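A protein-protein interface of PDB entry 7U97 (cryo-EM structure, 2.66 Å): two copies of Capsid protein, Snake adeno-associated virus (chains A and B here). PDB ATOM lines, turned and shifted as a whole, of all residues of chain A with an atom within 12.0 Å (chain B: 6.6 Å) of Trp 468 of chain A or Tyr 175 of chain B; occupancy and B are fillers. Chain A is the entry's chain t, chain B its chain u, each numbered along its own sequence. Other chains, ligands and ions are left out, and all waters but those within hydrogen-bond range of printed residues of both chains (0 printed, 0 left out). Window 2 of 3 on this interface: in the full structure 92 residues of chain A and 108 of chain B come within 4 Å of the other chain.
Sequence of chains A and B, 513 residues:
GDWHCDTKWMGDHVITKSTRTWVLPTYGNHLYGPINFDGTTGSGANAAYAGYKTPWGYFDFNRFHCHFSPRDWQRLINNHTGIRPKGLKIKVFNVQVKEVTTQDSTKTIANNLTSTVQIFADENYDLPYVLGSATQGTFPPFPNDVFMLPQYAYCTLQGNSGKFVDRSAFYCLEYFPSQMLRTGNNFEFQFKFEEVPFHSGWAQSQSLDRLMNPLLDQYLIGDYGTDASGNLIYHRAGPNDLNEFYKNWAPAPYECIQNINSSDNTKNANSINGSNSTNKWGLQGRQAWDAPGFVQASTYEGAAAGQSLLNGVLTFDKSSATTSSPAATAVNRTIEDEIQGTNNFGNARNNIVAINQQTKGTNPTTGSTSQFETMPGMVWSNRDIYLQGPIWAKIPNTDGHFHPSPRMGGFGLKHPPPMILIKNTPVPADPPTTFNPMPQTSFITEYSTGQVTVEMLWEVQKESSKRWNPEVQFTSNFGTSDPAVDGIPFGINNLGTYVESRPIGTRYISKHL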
ATOM      1  N   SER A 205       7.260  18.055  -7.391  1.00  0.00           N
ATOM      2  CA  SER A 205       6.419  17.217  -8.228  1.00  0.00           C
ATOM      3  C   SER A 205       6.562  15.731  -7.941  1.00  0.00           C
ATOM      4  O   SER A 205       5.939  14.924  -8.630  1.00  0.00           O
ATOM      5  CB  SER A 205       6.728  17.482  -9.697  1.00  0.00           C
ATOM      6  OG  SER A 205       8.070  17.158  -9.982  1.00  0.00           O
ATOM      7  N   GLU A 463      16.055  29.115 -13.866  1.00  0.00           N
ATOM      8  CA  GLU A 463      16.245  27.679 -13.990  1.00  0.00           C
ATOM      9  C   GLU A 463      15.913  27.240 -15.406  1.00  0.00           C
ATOM     10  O   GLU A 463      15.328  27.985 -16.191  1.00  0.00           O
ATOM     11  CB  GLU A 463      15.342  26.928 -13.010  1.00  0.00           C
ATOM     12  CG  GLU A 463      13.886  26.923 -13.462  1.00  0.00           C
ATOM     13  CD  GLU A 463      13.217  28.280 -13.323  1.00  0.00           C
ATOM     14  OE1 GLU A 463      13.888  29.246 -12.913  1.00  0.00           O
ATOM     15  OE2 GLU A 463      12.022  28.387 -13.651  1.00  0.00           O
ATOM     16  N   SER A 464      16.300  26.011 -15.728  1.00  0.00           N
ATOM     17  CA  SER A 464      15.853  25.351 -16.949  1.00  0.00           C
ATOM     18  C   SER A 464      15.319  23.979 -16.568  1.00  0.00           C
ATOM     19  O   SER A 464      16.080  23.113 -16.127  1.00  0.00           O
ATOM     20  CB  SER A 464      16.984  25.239 -17.969  1.00  0.00           C
ATOM     21  OG  SER A 464      18.034  24.425 -17.485  1.00  0.00           O
ATOM     22  N   SER A 465      14.018  23.781 -16.737  1.00  0.00           N
ATOM     23  CA  SER A 465      13.396  22.485 -16.532  1.00  0.00           C
ATOM     24  C   SER A 465      13.121  21.854 -17.882  1.00  0.00           C
ATOM     25  O   SER A 465      12.733  22.539 -18.829  1.00  0.00           O
ATOM     26  CB  SER A 465      12.090  22.601 -15.750  1.00  0.00           C
ATOM     27  OG  SER A 465      11.117  23.305 -16.496  1.00  0.00           O
ATOM     28  N   LYS A 466      13.353  20.553 -17.976  1.00  0.00           N
ATOM     29  CA  LYS A 466      13.107  19.828 -19.207  1.00  0.00           C
ATOM     30  C   LYS A 466      11.766  19.110 -19.231  1.00  0.00           C
ATOM     31  O   LYS A 466      11.544  18.286 -20.119  1.00  0.00           O
ATOM     32  CB  LYS A 466      14.259  18.878 -19.505  1.00  0.00           C
ATOM     33  CG  LYS A 466      15.503  19.665 -19.873  1.00  0.00           C
ATOM     34  CD  LYS A 466      16.616  18.814 -20.418  1.00  0.00           C
ATOM     35  CE  LYS A 466      16.299  18.349 -21.815  1.00  0.00           C
ATOM     36  NZ  LYS A 466      16.255  19.464 -22.780  1.00  0.00           N
ATOM     37  N   ARG A 467      10.887  19.356 -18.264  1.00  0.00           N
ATOM     38  CA  ARG A 467       9.535  18.842 -18.407  1.00  0.00           C
ATOM     39  C   ARG A 467       8.894  19.410 -19.664  1.00  0.00           C
ATOM     40  O   ARG A 467       9.194  20.523 -20.095  1.00  0.00           O
ATOM     41  CB  ARG A 467       8.670  19.172 -17.196  1.00  0.00           C
ATOM     42  CG  ARG A 467       8.436  20.630 -16.965  1.00  0.00           C
ATOM     43  CD  ARG A 467       7.530  20.844 -15.773  1.00  0.00           C
ATOM     44  NE  ARG A 467       6.142  20.491 -16.020  1.00  0.00           N
ATOM     45  CZ  ARG A 467       5.216  20.427 -15.071  1.00  0.00           C
ATOM     46  NH1 ARG A 467       5.541  20.649 -13.818  1.00  0.00           N
ATOM     47  NH2 ARG A 467       3.970  20.113 -15.367  1.00  0.00           N
ATOM     48  N   TRP A 468       8.010  18.616 -20.260  1.00  0.00           N
ATOM     49  CA  TRP A 468       7.371  18.936 -21.529  1.00  0.00           C
ATOM     50  C   TRP A 468       6.133  19.799 -21.315  1.00  0.00           C
ATOM     51  O   TRP A 468       6.048  20.915 -21.827  1.00  0.00           O
ATOM     52  CB  TRP A 468       7.022  17.636 -22.258  1.00  0.00           C
ATOM     53  CG  TRP A 468       6.462  17.814 -23.617  1.00  0.00           C
ATOM     54  CD1 TRP A 468       5.158  17.736 -23.978  1.00  0.00           C
ATOM     55  CD2 TRP A 468       7.195  18.061 -24.811  1.00  0.00           C
ATOM     56  NE1 TRP A 468       5.028  17.946 -25.322  1.00  0.00           N
ATOM     57  CE2 TRP A 468       6.270  18.144 -25.856  1.00  0.00           C
ATOM     58  CE3 TRP A 468       8.548  18.233 -25.095  1.00  0.00           C
ATOM     59  CZ2 TRP A 468       6.651  18.390 -27.159  1.00  0.00           C
ATOM     60  CZ3 TRP A 468       8.921  18.476 -26.387  1.00  0.00           C
ATOM     61  CH2 TRP A 468       7.982  18.554 -27.403  1.00  0.00           C
ATOM     62  N   ASN A 469       5.159  19.274 -20.580  1.00  0.00           N
ATOM     63  CA  ASN A 469       3.905  19.957 -20.327  1.00  0.00           C
ATOM     64  C   ASN A 469       4.120  21.274 -19.586  1.00  0.00           C
ATOM     65  O   ASN A 469       5.146  21.475 -18.937  1.00  0.00           O
ATOM     66  CB  ASN A 469       2.996  19.043 -19.519  1.00  0.00           C
ATOM     67  CG  ASN A 469       3.652  18.572 -18.259  1.00  0.00           C
ATOM     68  OD1 ASN A 469       4.861  18.657 -18.123  1.00  0.00           O
ATOM     69  ND2 ASN A 469       2.865  18.084 -17.323  1.00  0.00           N
ATOM     70  N   PRO A 470       3.161  22.188 -19.675  1.00  0.00           N
ATOM     71  CA  PRO A 470       3.272  23.472 -18.980  1.00  0.00           C
ATOM     72  C   PRO A 470       3.036  23.356 -17.478  1.00  0.00           C
ATOM     73  O   PRO A 470       2.544  22.354 -16.967  1.00  0.00           O
ATOM     74  CB  PRO A 470       2.187  24.313 -19.652  1.00  0.00           C
ATOM     75  CG  PRO A 470       1.233  23.354 -20.155  1.00  0.00           C
ATOM     76  CD  PRO A 470       2.018  22.179 -20.597  1.00  0.00           C
ATOM     77  N   GLU A 471       3.393  24.430 -16.775  1.00  0.00           N
ATOM     78  CA  GLU A 471       3.343  24.523 -15.324  1.00  0.00           C
ATOM     79  C   GLU A 471       2.290  25.520 -14.864  1.00  0.00           C
ATOM     80  O   GLU A 471       1.909  26.435 -15.590  1.00  0.00           O
ATOM     81  CB  GLU A 471       4.696  24.947 -14.759  1.00  0.00           C
ATOM     82  CG  GLU A 471       5.752  23.894 -14.851  1.00  0.00           C
ATOM     83  CD  GLU A 471       7.070  24.376 -14.332  1.00  0.00           C
ATOM     84  OE1 GLU A 471       7.202  25.597 -14.146  1.00  0.00           O
ATOM     85  OE2 GLU A 471       7.968  23.544 -14.095  1.00  0.00           O
ATOM     86  N   VAL A 472       1.818  25.327 -13.629  1.00  0.00           N
ATOM     87  CA  VAL A 472       0.871  26.266 -13.048  1.00  0.00           C
ATOM     88  C   VAL A 472       1.595  27.561 -12.732  1.00  0.00           C
ATOM     89  O   VAL A 472       2.779  27.568 -12.378  1.00  0.00           O
ATOM     90  CB  VAL A 472       0.198  25.709 -11.780  1.00  0.00           C
ATOM     91  CG1 VAL A 472      -0.454  24.388 -12.058  1.00  0.00           C
ATOM     92  CG2 VAL A 472       1.172  25.599 -10.660  1.00  0.00           C
ATOM     93  N   GLN A 473       0.883  28.671 -12.867  1.00  0.00           N
ATOM     94  CA  GLN A 473       1.468  29.973 -12.613  1.00  0.00           C
ATOM     95  C   GLN A 473       0.424  30.879 -11.991  1.00  0.00           C
ATOM     96  O   GLN A 473      -0.768  30.579 -11.989  1.00  0.00           O
ATOM     97  CB  GLN A 473       2.045  30.578 -13.885  1.00  0.00           C
ATOM     98  CG  GLN A 473       3.297  29.886 -14.331  1.00  0.00           C
ATOM     99  CD  GLN A 473       3.895  30.527 -15.522  1.00  0.00           C
ATOM    100  OE1 GLN A 473       3.205  31.180 -16.289  1.00  0.00           O
ATOM    101  NE2 GLN A 473       5.197  30.370 -15.682  1.00  0.00           N
ATOM    102  N   ILE A 509       6.486  26.707  -9.362  1.00  0.00           N
ATOM    103  CA  ILE A 509       7.194  25.914 -10.352  1.00  0.00           C
ATOM    104  C   ILE A 509       7.488  24.559  -9.745  1.00  0.00           C
ATOM    105  O   ILE A 509       7.982  24.471  -8.620  1.00  0.00           O
ATOM    106  CB  ILE A 509       8.485  26.602 -10.818  1.00  0.00           C
ATOM    107  CG1 ILE A 509       8.149  27.821 -11.662  1.00  0.00           C
ATOM    108  CG2 ILE A 509       9.341  25.655 -11.605  1.00  0.00           C
ATOM    109  CD1 ILE A 509       9.338  28.636 -12.007  1.00  0.00           C
ATOM    110  N   SER A 510       7.152  23.506 -10.471  1.00  0.00           N
ATOM    111  CA  SER A 510       7.404  22.165  -9.990  1.00  0.00           C
ATOM    112  C   SER A 510       8.828  21.754 -10.305  1.00  0.00           C
ATOM    113  O   SER A 510       9.409  22.164 -11.310  1.00  0.00           O
ATOM    114  CB  SER A 510       6.430  21.185 -10.621  1.00  0.00           C
ATOM    115  OG  SER A 510       5.112  21.498 -10.232  1.00  0.00           O
ATOM    116  N   LYS A 511       9.398  20.953  -9.419  1.00  0.00           N
ATOM    117  CA  LYS A 511      10.702  20.361  -9.643  1.00  0.00           C
ATOM    118  C   LYS A 511      10.701  18.981  -9.011  1.00  0.00           C
ATOM    119  O   LYS A 511      10.189  18.809  -7.906  1.00  0.00           O
ATOM    120  CB  LYS A 511      11.793  21.253  -9.065  1.00  0.00           C
ATOM    121  CG  LYS A 511      13.191  20.825  -9.376  1.00  0.00           C
ATOM    122  CD  LYS A 511      14.179  21.750  -8.709  1.00  0.00           C
ATOM    123  CE  LYS A 511      14.114  23.128  -9.319  1.00  0.00           C
ATOM    124  NZ  LYS A 511      15.101  24.037  -8.697  1.00  0.00           N
ATOM    125  N   HIS A 512      11.243  17.992  -9.712  1.00  0.00           N
ATOM    126  CA  HIS A 512      11.221  16.637  -9.183  1.00  0.00           C
ATOM    127  C   HIS A 512      12.085  16.548  -7.935  1.00  0.00           C
ATOM    128  O   HIS A 512      13.139  17.179  -7.839  1.00  0.00           O
ATOM    129  CB  HIS A 512      11.695  15.626 -10.221  1.00  0.00           C
ATOM    130  CG  HIS A 512      13.094  15.850 -10.687  1.00  0.00           C
ATOM    131  ND1 HIS A 512      13.419  16.795 -11.631  1.00  0.00           N
ATOM    132  CD2 HIS A 512      14.257  15.266 -10.322  1.00  0.00           C
ATOM    133  CE1 HIS A 512      14.721  16.774 -11.838  1.00  0.00           C
ATOM    134  NE2 HIS A 512      15.253  15.856 -11.056  1.00  0.00           N
ATOM    135  N   TYR B  32       5.846   5.831 -25.436  1.00  0.00           N
ATOM    136  CA  TYR B  32       5.618   6.193 -24.051  1.00  0.00           C
ATOM    137  C   TYR B  32       4.246   5.698 -23.636  1.00  0.00           C
ATOM    138  O   TYR B  32       3.388   5.427 -24.477  1.00  0.00           O
ATOM    139  CB  TYR B  32       5.684   7.704 -23.876  1.00  0.00           C
ATOM    140  CG  TYR B  32       7.046   8.315 -24.017  1.00  0.00           C
ATOM    141  CD1 TYR B  32       7.801   8.617 -22.905  1.00  0.00           C
ATOM    142  CD2 TYR B  32       7.584   8.571 -25.256  1.00  0.00           C
ATOM    143  CE1 TYR B  32       9.042   9.180 -23.026  1.00  0.00           C
ATOM    144  CE2 TYR B  32       8.826   9.129 -25.383  1.00  0.00           C
ATOM    145  CZ  TYR B  32       9.551   9.433 -24.267  1.00  0.00           C
ATOM    146  OH  TYR B  32      10.793   9.991 -24.389  1.00  0.00           O
ATOM    147  N   ALA B 169       4.504  15.995 -13.930  1.00  0.00           N
ATOM    148  CA  ALA B 169       5.375  16.320 -15.043  1.00  0.00           C
ATOM    149  C   ALA B 169       5.458  15.163 -16.024  1.00  0.00           C
ATOM    150  O   ALA B 169       5.407  13.996 -15.644  1.00  0.00           O
ATOM    151  CB  ALA B 169       6.777  16.670 -14.557  1.00  0.00           C
ATOM    152  N   PHE B 170       5.582  15.509 -17.297  1.00  0.00           N
ATOM    153  CA  PHE B 170       5.859  14.565 -18.366  1.00  0.00           C
ATOM    154  C   PHE B 170       7.158  14.975 -19.032  1.00  0.00           C
ATOM    155  O   PHE B 170       7.309  16.125 -19.447  1.00  0.00           O
ATOM    156  CB  PHE B 170       4.716  14.528 -19.376  1.00  0.00           C
ATOM    157  CG  PHE B 170       5.045  13.793 -20.625  1.00  0.00           C
ATOM    158  CD1 PHE B 170       5.078  12.422 -20.650  1.00  0.00           C
ATOM    159  CD2 PHE B 170       5.309  14.479 -21.789  1.00  0.00           C
ATOM    160  CE1 PHE B 170       5.383  11.750 -21.801  1.00  0.00           C
ATOM    161  CE2 PHE B 170       5.613  13.807 -22.945  1.00  0.00           C
ATOM    162  CZ  PHE B 170       5.648  12.443 -22.948  1.00  0.00           C
ATOM    163  N   TYR B 171       8.100  14.046 -19.111  1.00  0.00           N
ATOM    164  CA  TYR B 171       9.427  14.318 -19.640  1.00  0.00           C
ATOM    165  C   TYR B 171       9.600  13.576 -20.954  1.00  0.00           C
ATOM    166  O   TYR B 171       9.495  12.349 -20.994  1.00  0.00           O
ATOM    167  CB  TYR B 171      10.502  13.887 -18.648  1.00  0.00           C
ATOM    168  CG  TYR B 171      10.441  14.600 -17.328  1.00  0.00           C
ATOM    169  CD1 TYR B 171      11.066  15.814 -17.151  1.00  0.00           C
ATOM    170  CD2 TYR B 171       9.765  14.050 -16.260  1.00  0.00           C
ATOM    171  CE1 TYR B 171      11.012  16.463 -15.954  1.00  0.00           C
ATOM    172  CE2 TYR B 171       9.707  14.693 -15.061  1.00  0.00           C
ATOM    173  CZ  TYR B 171      10.332  15.901 -14.914  1.00  0.00           C
ATOM    174  OH  TYR B 171      10.280  16.554 -13.710  1.00  0.00           O
ATOM    175  N   CYS B 172       9.861  14.318 -22.022  1.00  0.00           N
ATOM    176  CA  CYS B 172      10.251  13.730 -23.292  1.00  0.00           C
ATOM    177  C   CYS B 172      11.762  13.574 -23.306  1.00  0.00           C
ATOM    178  O   CYS B 172      12.492  14.540 -23.077  1.00  0.00           O
ATOM    179  CB  CYS B 172       9.796  14.601 -24.460  1.00  0.00           C
ATOM    180  SG  CYS B 172      10.170  13.946 -26.090  1.00  0.00           S
ATOM    181  N   LEU B 173      12.230  12.360 -23.554  1.00  0.00           N
ATOM    182  CA  LEU B 173      13.651  12.080 -23.467  1.00  0.00           C
ATOM    183  C   LEU B 173      14.372  12.228 -24.795  1.00  0.00           C
ATOM    184  O   LEU B 173      15.595  12.096 -24.834  1.00  0.00           O
ATOM    185  CB  LEU B 173      13.874  10.674 -22.911  1.00  0.00           C
ATOM    186  CG  LEU B 173      13.873  10.517 -21.392  1.00  0.00           C
ATOM    187  CD1 LEU B 173      12.520  10.804 -20.780  1.00  0.00           C
ATOM    188  CD2 LEU B 173      14.290   9.134 -21.055  1.00  0.00           C
ATOM    189  N   GLU B 174      13.657  12.495 -25.876  1.00  0.00           N
ATOM    190  CA  GLU B 174      14.287  12.851 -27.136  1.00  0.00           C
ATOM    191  C   GLU B 174      14.529  14.339 -27.245  1.00  0.00           C
ATOM    192  O   GLU B 174      14.996  14.806 -28.285  1.00  0.00           O
ATOM    193  CB  GLU B 174      13.436  12.381 -28.314  1.00  0.00           C
ATOM    194  CG  GLU B 174      13.371  10.881 -28.450  1.00  0.00           C
ATOM    195  CD  GLU B 174      12.339  10.266 -27.547  1.00  0.00           C
ATOM    196  OE1 GLU B 174      11.676  11.015 -26.808  1.00  0.00           O
ATOM    197  OE2 GLU B 174      12.198   9.031 -27.566  1.00  0.00           O
ATOM    198  N   TYR B 175      14.238  15.067 -26.177  1.00  0.00           N
ATOM    199  CA  TYR B 175      14.465  16.498 -26.152  1.00  0.00           C
ATOM    200  C   TYR B 175      15.826  16.746 -25.550  1.00  0.00           C
ATOM    201  O   TYR B 175      16.138  17.863 -25.151  1.00  0.00           O
ATOM    202  CB  TYR B 175      13.392  17.162 -25.308  1.00  0.00           C
ATOM    203  CG  TYR B 175      13.034  18.569 -25.723  1.00  0.00           C
ATOM    204  CD1 TYR B 175      12.286  18.800 -26.865  1.00  0.00           C
ATOM    205  CD2 TYR B 175      13.424  19.660 -24.960  1.00  0.00           C
ATOM    206  CE1 TYR B 175      11.946  20.082 -27.245  1.00  0.00           C
ATOM    207  CE2 TYR B 175      13.088  20.946 -25.333  1.00  0.00           C
ATOM    208  CZ  TYR B 175      12.348  21.151 -26.477  1.00  0.00           C
ATOM    209  OH  TYR B 175      12.005  22.426 -26.856  1.00  0.00           O
ATOM    210  N   PHE B 176      16.637  15.701 -25.469  1.00  0.00           N
ATOM    211  CA  PHE B 176      17.967  15.818 -24.897  1.00  0.00           C
ATOM    212  C   PHE B 176      18.994  15.573 -25.978  1.00  0.00           C
ATOM    213  O   PHE B 176      18.795  14.725 -26.843  1.00  0.00           O
ATOM    214  CB  PHE B 176      18.176  14.789 -23.792  1.00  0.00           C
ATOM    215  CG  PHE B 176      17.287  14.971 -22.598  1.00  0.00           C
ATOM    216  CD1 PHE B 176      17.825  15.307 -21.369  1.00  0.00           C
ATOM    217  CD2 PHE B 176      15.919  14.787 -22.697  1.00  0.00           C
ATOM    218  CE1 PHE B 176      17.016  15.466 -20.261  1.00  0.00           C
ATOM    219  CE2 PHE B 176      15.103  14.947 -21.596  1.00  0.00           C
ATOM    220  CZ  PHE B 176      15.652  15.288 -20.375  1.00  0.00           C
ATOM    221  N   PRO B 177      20.102  16.316 -25.945  1.00  0.00           N
ATOM    222  CA  PRO B 177      21.165  16.036 -26.908  1.00  0.00           C
ATOM    223  C   PRO B 177      21.784  14.677 -26.622  1.00  0.00           C
ATOM    224  O   PRO B 177      22.200  14.434 -25.493  1.00  0.00           O
ATOM    225  CB  PRO B 177      22.175  17.151 -26.643  1.00  0.00           C
ATOM    226  CG  PRO B 177      21.394  18.237 -25.980  1.00  0.00           C
ATOM    227  CD  PRO B 177      20.369  17.527 -25.153  1.00  0.00           C
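The backbone NH of Trp 468 of chain A is in hydrogen-bond range of the backbone carbonyl oxygen of Phe 170 of chain B. N of Phe 170 of chain B is in hydrogen-bond range of OD1 of Asn 469 of chain A, 3.3 Å away. The side-chain amino group (NZ) of Lys 466 of chain A is in hydrogen-bond range of the backbone carbonyl oxygen (O) of Tyr 175 of chain B (2.9 Å).
The side-chain sulfur (SG) of Cys 172 of chain B sits at hydrogen-bond distance from the side-chain carboxylate (OE1) of Glu 174 of chain B, 3.4 Å away. The guanidinium group (NH1) of Arg 467 of chain A lies within salt-bridge range of the side-chain carboxylate (OE2) of Glu 471 of chain A (3.8 Å). N of His 512 of chain A sits at hydrogen-bond distance from OG of Ser 205 of chain A. The guanidinium group of Arg 467 of chain A lies close to the side-chain amide nitrogen of Asn 469 of chain A, 3.0 Å away. O of Pro 470 of chain A is in hydrogen-bond range of NH2 of Arg 467 of chain A (3.1 Å).
O of Lys 466 of chain A touches CD1 of Tyr 171 of chain B, 3.9 Å away. Lys 466 of chain A touches Phe 176 of chain B. O of Phe 170 of chain B touches C of Arg 467 of chain A, 3.7 Å away. Arg 467 of chain A touches Tyr 171 of chain B. Trp 468 of chain A touches Cys 172 of chain B (CE3 to CB, 3.9 Å). CD1 of Tyr 175 of chain B touches CZ3 of Trp 468 of chain A, at 3.4 Å. Asn 469 of chain A touches Ala 169 of chain B (ND2 to CA, 3.8 Å). ND1 of His 512 of chain A touches OH of Tyr 171 of chain B, at 3.8 Å.
Of chain B, only Phe 170 (2.7 Å), Cys 172 (3.9 Å) and Tyr 175 (3.4 Å) come within 4 Å of Trp 468 of chain A. Tyr 175 of chain B touches just these residues of chain A: Lys 466 and Trp 468. Ala 169 of chain B touches just one residue of chain A: Asn 469. Phe 170 of chain B touches just these residues of chain A: Arg 467, Trp 468 and Asn 469. Cys 172 of chain B touches one residue of chain A. Leu 173 of chain B touches none of the printed residues of chain A. Printed residues of chain A within 4 Å of Phe 176 of chain B: Lys 466 (3.4 Å). No residue of chain A comes within 4 Å of Pro 177 of chain B. Printed residues of chain B within 4 Å of His 512 of chain A: Tyr 171 (3.8 Å). Printed residues of chain B within 4 Å of Lys 466 of chain A: Tyr 171, Tyr 175 and Phe 176. Of the printed residues of chain B, Asn 469 of chain A touches Ala 169 and Phe 170. Printed residues of chain B within 4 Å of Arg 467 of chain A: Phe 170 and Tyr 171. Gln 473 of chain A touches none of the printed residues of chain B. The nearest printed residue of chain B that does not touch His 512 of chain A is Ala 169 of chain B (6.6 Å).
Hydrophobic or aromatic side chains of chain B within 4 Å of the printed part of chain A: Phe 170, Tyr 171, Tyr 175 and Phe 176. Along chain B the printed residues that touch a printed residue of chain A span positions 169 to 176.
No position is printed for both chains.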
